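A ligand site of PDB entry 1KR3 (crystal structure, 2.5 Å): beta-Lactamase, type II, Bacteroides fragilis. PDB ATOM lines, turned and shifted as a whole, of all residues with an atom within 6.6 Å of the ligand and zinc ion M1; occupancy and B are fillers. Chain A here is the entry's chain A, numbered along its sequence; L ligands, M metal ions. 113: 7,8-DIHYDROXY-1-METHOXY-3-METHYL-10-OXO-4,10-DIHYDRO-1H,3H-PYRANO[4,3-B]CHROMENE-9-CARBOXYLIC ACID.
The side-chain sulfur (SG) of Cys 164 lies close to an oxygen (O19) of the ligand, 3.8 Å away.
NZ of Lys 167 lies within salt-bridge range of O30 of the ligand, 3.97 Å away.
N of Asn 176 sits close to O30 of the ligand (3.5 Å).
The side-chain amide nitrogen (ND2) of Asn 176 is in hydrogen-bond range of an oxygen (O16) of the ligand.
ND1 of His 206 is in hydrogen-bond range of O of Pro 36 (2.5 Å).
A ring nitrogen (NE2) of His 206 lies within hydrogen-bond range of the side-chain carboxylate (OD2) of Asp 86, 3.0 Å away.
NZ of Lys 167 lies close to O of Ile 174 (3.3 Å).
Residues that only touch the ligand: His 206, His 145 and Ile 29.
Six residues have an atom within 4 Å of the ligand: Ile 29, His 145, Cys 164, Lys 167, Asn 176 and His 206.
The nearest printed residue that does not touch the ligand is Ser 173 (4.04 Å).
Asp 86 touches zinc ion M1 (OD2 to ZN, 3.0 Å).
His 206 touches zinc ion M1.
Zinc ion M1 is bound by the side-chain sulfur (SG) of Cys 164 (2.1 Å).
Zinc ion M1 has one donor atom within binding distance.
Slightly farther from zinc ion M1 lies O19 of the ligand (2.6 Å).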
ATOM      1  N   ILE A  29      23.572   4.849 -14.389  1.00  0.00           N
ATOM      2  CA  ILE A  29      24.139   4.353 -13.147  1.00  0.00           C
ATOM      3  C   ILE A  29      23.659   2.918 -12.899  1.00  0.00           C
ATOM      4  O   ILE A  29      22.465   2.670 -12.819  1.00  0.00           O
ATOM      5  CB  ILE A  29      23.801   5.276 -11.942  1.00  0.00           C
ATOM      6  CG1 ILE A  29      24.329   6.688 -12.236  1.00  0.00           C
ATOM      7  CG2 ILE A  29      24.477   4.750 -10.665  1.00  0.00           C
ATOM      8  CD1 ILE A  29      24.087   7.682 -11.125  1.00  0.00           C
ATOM      9  N   GLY A  33      19.511   3.282 -13.634  1.00  0.00           N
ATOM     10  CA  GLY A  33      19.283   3.648 -15.020  1.00  0.00           C
ATOM     11  C   GLY A  33      19.620   5.060 -15.462  1.00  0.00           C
ATOM     12  O   GLY A  33      20.385   5.763 -14.815  1.00  0.00           O
ATOM     13  N   MET A  34      19.044   5.450 -16.604  1.00  0.00           N
ATOM     14  CA  MET A  34      19.193   6.784 -17.182  1.00  0.00           C
ATOM     15  C   MET A  34      18.744   7.829 -16.166  1.00  0.00           C
ATOM     16  O   MET A  34      17.538   8.034 -15.982  1.00  0.00           O
ATOM     17  CB  MET A  34      18.294   6.917 -18.433  1.00  0.00           C
ATOM     18  CG  MET A  34      18.917   6.652 -19.805  1.00  0.00           C
ATOM     19  SD  MET A  34      20.144   7.910 -20.275  1.00  0.00           S
ATOM     20  CE  MET A  34      19.211   9.456 -19.973  1.00  0.00           C
ATOM     21  N   VAL A  35      19.677   8.500 -15.508  1.00  0.00           N
ATOM     22  CA  VAL A  35      19.284   9.507 -14.535  1.00  0.00           C
ATOM     23  C   VAL A  35      20.019  10.855 -14.613  1.00  0.00           C
ATOM     24  O   VAL A  35      21.224  10.887 -14.843  1.00  0.00           O
ATOM     25  CB  VAL A  35      19.375   8.933 -13.092  1.00  0.00           C
ATOM     26  CG1 VAL A  35      18.661   7.599 -13.039  1.00  0.00           C
ATOM     27  CG2 VAL A  35      20.810   8.790 -12.648  1.00  0.00           C
ATOM     28  N   PRO A  36      19.269  11.968 -14.512  1.00  0.00           N
ATOM     29  CA  PRO A  36      19.649  13.387 -14.541  1.00  0.00           C
ATOM     30  C   PRO A  36      20.226  13.961 -13.235  1.00  0.00           C
ATOM     31  O   PRO A  36      19.557  13.935 -12.210  1.00  0.00           O
ATOM     32  CB  PRO A  36      18.329  14.067 -14.883  1.00  0.00           C
ATOM     33  CG  PRO A  36      17.383  13.266 -14.084  1.00  0.00           C
ATOM     34  CD  PRO A  36      17.796  11.874 -14.551  1.00  0.00           C
ATOM     35  N   SER A  37      21.454  14.491 -13.286  1.00  0.00           N
ATOM     36  CA  SER A  37      22.081  15.074 -12.101  1.00  0.00           C
ATOM     37  C   SER A  37      22.304  16.560 -12.317  1.00  0.00           C
ATOM     38  O   SER A  37      22.744  16.964 -13.396  1.00  0.00           O
ATOM     39  CB  SER A  37      23.454  14.434 -11.814  1.00  0.00           C
ATOM     40  OG  SER A  37      23.371  13.064 -11.499  1.00  0.00           O
ATOM     41  N   HIS A  82      28.838  16.389  -1.915  1.00  0.00           N
ATOM     42  CA  HIS A  82      29.324  15.299  -1.096  1.00  0.00           C
ATOM     43  C   HIS A  82      30.225  14.371  -1.941  1.00  0.00           C
ATOM     44  O   HIS A  82      30.484  14.657  -3.109  1.00  0.00           O
ATOM     45  CB  HIS A  82      28.178  14.508  -0.382  1.00  0.00           C
ATOM     46  CG  HIS A  82      27.061  14.054  -1.280  1.00  0.00           C
ATOM     47  ND1 HIS A  82      26.134  14.887  -1.840  1.00  0.00           N
ATOM     48  CD2 HIS A  82      26.835  12.829  -1.816  1.00  0.00           C
ATOM     49  CE1 HIS A  82      25.397  14.169  -2.703  1.00  0.00           C
ATOM     50  NE2 HIS A  82      25.773  12.907  -2.735  1.00  0.00           N
ATOM     51  N   HIS A  84      29.840  11.546  -3.511  1.00  0.00           N
ATOM     52  CA  HIS A  84      29.371  10.690  -4.594  1.00  0.00           C
ATOM     53  C   HIS A  84      29.783  11.028  -6.027  1.00  0.00           C
ATOM     54  O   HIS A  84      30.324  12.114  -6.303  1.00  0.00           O
ATOM     55  CB  HIS A  84      27.860  10.492  -4.511  1.00  0.00           C
ATOM     56  CG  HIS A  84      27.453   9.515  -3.455  1.00  0.00           C
ATOM     57  ND1 HIS A  84      26.191   9.520  -2.926  1.00  0.00           N
ATOM     58  CD2 HIS A  84      28.165   8.519  -2.885  1.00  0.00           C
ATOM     59  CE1 HIS A  84      26.164   8.533  -2.046  1.00  0.00           C
ATOM     60  NE2 HIS A  84      27.335   7.895  -1.988  1.00  0.00           N
ATOM     61  N   ASP A  86      28.089  11.698  -8.693  1.00  0.00           N
ATOM     62  CA  ASP A  86      27.417  12.825  -9.312  1.00  0.00           C
ATOM     63  C   ASP A  86      27.725  14.186  -8.645  1.00  0.00           C
ATOM     64  O   ASP A  86      26.984  15.173  -8.804  1.00  0.00           O
ATOM     65  CB  ASP A  86      25.916  12.521  -9.407  1.00  0.00           C
ATOM     66  CG  ASP A  86      25.286  12.217  -8.057  1.00  0.00           C
ATOM     67  OD1 ASP A  86      25.865  11.412  -7.298  1.00  0.00           O
ATOM     68  OD2 ASP A  86      24.189  12.769  -7.767  1.00  0.00           O
ATOM     69  N   CYS A  87      28.848  14.248  -7.932  1.00  0.00           N
ATOM     70  CA  CYS A  87      29.285  15.475  -7.293  1.00  0.00           C
ATOM     71  C   CYS A  87      30.789  15.717  -7.665  1.00  0.00           C
ATOM     72  O   CYS A  87      31.161  16.833  -8.047  1.00  0.00           O
ATOM     73  CB  CYS A  87      29.105  15.377  -5.767  1.00  0.00           C
ATOM     74  SG  CYS A  87      27.396  14.943  -5.180  1.00  0.00           S
ATOM     75  N   HIS A 145      21.253  13.083   3.144  1.00  0.00           N
ATOM     76  CA  HIS A 145      21.335  12.086   2.082  1.00  0.00           C
ATOM     77  C   HIS A 145      22.592  11.264   2.280  1.00  0.00           C
ATOM     78  O   HIS A 145      22.612  10.074   2.043  1.00  0.00           O
ATOM     79  CB  HIS A 145      21.425  12.769   0.723  1.00  0.00           C
ATOM     80  CG  HIS A 145      21.937  11.877  -0.362  1.00  0.00           C
ATOM     81  ND1 HIS A 145      21.143  10.950  -1.003  1.00  0.00           N
ATOM     82  CD2 HIS A 145      23.194  11.702  -0.840  1.00  0.00           C
ATOM     83  CE1 HIS A 145      21.901  10.230  -1.825  1.00  0.00           C
ATOM     84  NE2 HIS A 145      23.143  10.668  -1.744  1.00  0.00           N
ATOM     85  N   GLY A 163      21.441  20.289  -3.157  1.00  0.00           N
ATOM     86  CA  GLY A 163      21.992  18.975  -3.362  1.00  0.00           C
ATOM     87  C   GLY A 163      20.940  17.895  -3.139  1.00  0.00           C
ATOM     88  O   GLY A 163      19.749  18.168  -3.031  1.00  0.00           O
ATOM     89  N   CYS A 164      21.410  16.664  -3.021  1.00  0.00           N
ATOM     90  CA  CYS A 164      20.542  15.523  -2.838  1.00  0.00           C
ATOM     91  C   CYS A 164      19.906  15.379  -1.463  1.00  0.00           C
ATOM     92  O   CYS A 164      19.174  14.421  -1.236  1.00  0.00           O
ATOM     93  CB  CYS A 164      21.308  14.257  -3.215  1.00  0.00           C
ATOM     94  SG  CYS A 164      22.093  14.512  -4.819  1.00  0.00           S
ATOM     95  N   MET A 165      20.148  16.297  -0.550  1.00  0.00           N
ATOM     96  CA  MET A 165      19.431  16.163   0.722  1.00  0.00           C
ATOM     97  C   MET A 165      18.037  16.680   0.408  1.00  0.00           C
ATOM     98  O   MET A 165      17.104  16.392   1.127  1.00  0.00           O
ATOM     99  CB  MET A 165      20.038  16.986   1.897  1.00  0.00           C
ATOM    100  CG  MET A 165      19.659  18.457   1.971  1.00  0.00           C
ATOM    101  SD  MET A 165      20.343  19.211   3.468  1.00  0.00           S
ATOM    102  CE  MET A 165      22.221  19.009   3.258  1.00  0.00           C
ATOM    103  N   LYS A 167      14.774  16.704  -2.139  1.00  0.00           N
ATOM    104  CA  LYS A 167      14.079  16.018  -3.237  1.00  0.00           C
ATOM    105  C   LYS A 167      13.154  17.008  -4.042  1.00  0.00           C
ATOM    106  O   LYS A 167      12.700  18.028  -3.494  1.00  0.00           O
ATOM    107  CB  LYS A 167      13.225  14.891  -2.650  1.00  0.00           C
ATOM    108  CG  LYS A 167      13.781  13.508  -2.780  1.00  0.00           C
ATOM    109  CD  LYS A 167      14.752  13.173  -1.749  1.00  0.00           C
ATOM    110  CE  LYS A 167      15.204  11.746  -1.945  1.00  0.00           C
ATOM    111  NZ  LYS A 167      15.781  11.538  -3.309  1.00  0.00           N
ATOM    112  N   ASP A 168      12.880  16.694  -5.319  1.00  0.00           N
ATOM    113  CA  ASP A 168      12.035  17.566  -6.132  1.00  0.00           C
ATOM    114  C   ASP A 168      10.557  17.279  -5.925  1.00  0.00           C
ATOM    115  O   ASP A 168      10.184  16.152  -5.584  1.00  0.00           O
ATOM    116  CB  ASP A 168      12.373  17.501  -7.643  1.00  0.00           C
ATOM    117  CG  ASP A 168      11.940  16.201  -8.337  1.00  0.00           C
ATOM    118  OD1 ASP A 168      12.719  15.200  -8.394  1.00  0.00           O
ATOM    119  OD2 ASP A 168      10.811  16.184  -8.850  1.00  0.00           O
ATOM    120  N   ALA A 171       8.754  13.998  -6.559  1.00  0.00           N
ATOM    121  CA  ALA A 171       9.294  12.742  -6.056  1.00  0.00           C
ATOM    122  C   ALA A 171       8.511  12.183  -4.864  1.00  0.00           C
ATOM    123  O   ALA A 171       8.281  12.845  -3.844  1.00  0.00           O
ATOM    124  CB  ALA A 171      10.765  12.904  -5.699  1.00  0.00           C
ATOM    125  N   THR A 172       8.124  10.917  -5.013  1.00  0.00           N
ATOM    126  CA  THR A 172       7.365  10.181  -4.016  1.00  0.00           C
ATOM    127  C   THR A 172       8.269   9.182  -3.253  1.00  0.00           C
ATOM    128  O   THR A 172       7.946   8.725  -2.143  1.00  0.00           O
ATOM    129  CB  THR A 172       6.234   9.419  -4.748  1.00  0.00           C
ATOM    130  OG1 THR A 172       6.794   8.630  -5.818  1.00  0.00           O
ATOM    131  CG2 THR A 172       5.238  10.392  -5.357  1.00  0.00           C
ATOM    132  N   SER A 173       9.393   8.863  -3.880  1.00  0.00           N
ATOM    133  CA  SER A 173      10.402   7.935  -3.350  1.00  0.00           C
ATOM    134  C   SER A 173      11.555   8.598  -2.593  1.00  0.00           C
ATOM    135  O   SER A 173      11.978   9.714  -2.904  1.00  0.00           O
ATOM    136  CB  SER A 173      10.969   7.106  -4.511  1.00  0.00           C
ATOM    137  OG  SER A 173      12.298   6.666  -4.260  1.00  0.00           O
ATOM    138  N   ILE A 174      12.075   7.906  -1.584  1.00  0.00           N
ATOM    139  CA  ILE A 174      13.178   8.448  -0.832  1.00  0.00           C
ATOM    140  C   ILE A 174      14.411   8.122  -1.621  1.00  0.00           C
ATOM    141  O   ILE A 174      15.431   8.797  -1.492  1.00  0.00           O
ATOM    142  CB  ILE A 174      13.265   7.842   0.568  1.00  0.00           C
ATOM    143  CG1 ILE A 174      14.480   8.409   1.282  1.00  0.00           C
ATOM    144  CG2 ILE A 174      13.299   6.336   0.506  1.00  0.00           C
ATOM    145  CD1 ILE A 174      14.605   8.004   2.711  1.00  0.00           C
ATOM    146  N   ASN A 176      17.806   6.461  -3.150  1.00  0.00           N
ATOM    147  CA  ASN A 176      19.130   5.952  -2.741  1.00  0.00           C
ATOM    148  C   ASN A 176      19.667   6.284  -1.337  1.00  0.00           C
ATOM    149  O   ASN A 176      20.479   7.217  -1.180  1.00  0.00           O
ATOM    150  CB  ASN A 176      20.148   6.424  -3.801  1.00  0.00           C
ATOM    151  CG  ASN A 176      21.541   5.914  -3.541  1.00  0.00           C
ATOM    152  OD1 ASN A 176      21.762   4.702  -3.457  1.00  0.00           O
ATOM    153  ND2 ASN A 176      22.492   6.839  -3.429  1.00  0.00           N
ATOM    154  N   ILE A 177      19.275   5.484  -0.327  1.00  0.00           N
ATOM    155  CA  ILE A 177      19.704   5.723   1.054  1.00  0.00           C
ATOM    156  C   ILE A 177      20.846   4.832   1.600  1.00  0.00           C
ATOM    157  O   ILE A 177      20.908   4.540   2.790  1.00  0.00           O
ATOM    158  CB  ILE A 177      18.495   5.613   2.004  1.00  0.00           C
ATOM    159  CG1 ILE A 177      17.994   4.170   2.130  1.00  0.00           C
ATOM    160  CG2 ILE A 177      17.356   6.426   1.470  1.00  0.00           C
ATOM    161  CD1 ILE A 177      16.834   4.035   3.115  1.00  0.00           C
ATOM    162  N   TRP A 185      18.710  13.250   9.104  1.00  0.00           N
ATOM    163  CA  TRP A 185      18.086  13.899   7.984  1.00  0.00           C
ATOM    164  C   TRP A 185      17.008  14.909   8.347  1.00  0.00           C
ATOM    165  O   TRP A 185      17.063  16.074   7.910  1.00  0.00           O
ATOM    166  CB  TRP A 185      17.573  12.864   7.013  1.00  0.00           C
ATOM    167  CG  TRP A 185      17.558  13.381   5.598  1.00  0.00           C
ATOM    168  CD1 TRP A 185      17.425  14.689   5.202  1.00  0.00           C
ATOM    169  CD2 TRP A 185      17.557  12.603   4.394  1.00  0.00           C
ATOM    170  NE1 TRP A 185      17.334  14.766   3.849  1.00  0.00           N
ATOM    171  CE2 TRP A 185      17.406  13.502   3.315  1.00  0.00           C
ATOM    172  CE3 TRP A 185      17.661  11.223   4.130  1.00  0.00           C
ATOM    173  CZ2 TRP A 185      17.353  13.071   1.989  1.00  0.00           C
ATOM    174  CZ3 TRP A 185      17.599  10.800   2.809  1.00  0.00           C
ATOM    175  CH2 TRP A 185      17.449  11.720   1.753  1.00  0.00           C
ATOM    176  N   GLY A 205      19.401  18.034  -5.915  1.00  0.00           N
ATOM    177  CA  GLY A 205      20.394  17.234  -6.599  1.00  0.00           C
ATOM    178  C   GLY A 205      19.861  16.576  -7.848  1.00  0.00           C
ATOM    179  O   GLY A 205      20.648  16.321  -8.789  1.00  0.00           O
ATOM    180  N   HIS A 206      18.542  16.284  -7.869  1.00  0.00           N
ATOM    181  CA  HIS A 206      17.889  15.635  -9.037  1.00  0.00           C
ATOM    182  C   HIS A 206      16.501  16.197  -9.173  1.00  0.00           C
ATOM    183  O   HIS A 206      15.797  16.357  -8.180  1.00  0.00           O
ATOM    184  CB  HIS A 206      17.824  14.115  -8.845  1.00  0.00           C
ATOM    185  CG  HIS A 206      19.176  13.479  -8.777  1.00  0.00           C
ATOM    186  ND1 HIS A 206      19.915  13.151  -9.903  1.00  0.00           N
ATOM    187  CD2 HIS A 206      19.984  13.237  -7.723  1.00  0.00           C
ATOM    188  CE1 HIS A 206      21.106  12.728  -9.543  1.00  0.00           C
ATOM    189  NE2 HIS A 206      21.177  12.776  -8.221  1.00  0.00           N
ATOM    190  N   GLY A 207      16.130  16.527 -10.400  1.00  0.00           N
ATOM    191  CA  GLY A 207      14.800  17.073 -10.613  1.00  0.00           C
ATOM    192  C   GLY A 207      14.652  18.557 -10.812  1.00  0.00           C
ATOM    193  O   GLY A 207      15.627  19.306 -10.920  1.00  0.00           O
HETATM  194  C1  113 L   1      21.412   7.863  -7.486  1.00  0.00           C
HETATM  195  C2  113 L   1      20.306   7.395  -8.206  1.00  0.00           C
HETATM  196  C3  113 L   1      19.122   8.121  -8.155  1.00  0.00           C
HETATM  197  C4  113 L   1      18.985   9.179  -7.246  1.00  0.00           C
HETATM  198  C5  113 L   1      19.957   9.339  -6.225  1.00  0.00           C
HETATM  199  C6  113 L   1      21.231   8.751  -6.423  1.00  0.00           C
HETATM  200  O8  113 L   1      18.087   7.801  -9.017  1.00  0.00           O
HETATM  201  C9  113 L   1      16.891   8.492  -9.022  1.00  0.00           C
HETATM  202  C10 113 L   1      16.697   9.612  -8.288  1.00  0.00           C
HETATM  203  C11 113 L   1      17.835  10.083  -7.402  1.00  0.00           C
HETATM  204  C12 113 L   1      15.824   7.906  -9.903  1.00  0.00           C
HETATM  205  C13 113 L   1      14.414   8.294  -9.388  1.00  0.00           C
HETATM  206  O14 113 L   1      14.342   9.697  -9.108  1.00  0.00           O
HETATM  207  C15 113 L   1      15.354  10.354  -8.339  1.00  0.00           C
HETATM  208  O16 113 L   1      22.349   8.988  -5.630  1.00  0.00           O
HETATM  209  O17 113 L   1      22.704   7.484  -7.804  1.00  0.00           O
HETATM  210  C18 113 L   1      19.664  10.080  -4.975  1.00  0.00           C
HETATM  211  O19 113 L   1      19.964  11.388  -5.003  1.00  0.00           O
HETATM  212  O20 113 L   1      14.871  10.739  -7.052  1.00  0.00           O
HETATM  213  C22 113 L   1      14.414   9.770  -6.122  1.00  0.00           C
HETATM  214  C26 113 L   1      13.294   7.927 -10.374  1.00  0.00           C
HETATM  215  O30 113 L   1      19.143   9.542  -4.014  1.00  0.00           O
HETATM  216  O31 113 L   1      17.749  11.177  -6.876  1.00  0.00           O
HETATM  217 ZN    ZN M   1      22.269  12.575  -5.491  1.00  0.00          ZN
HETATM  218 ZN    ZN M   2      24.677  11.249  -3.495  1.00  0.00          ZN
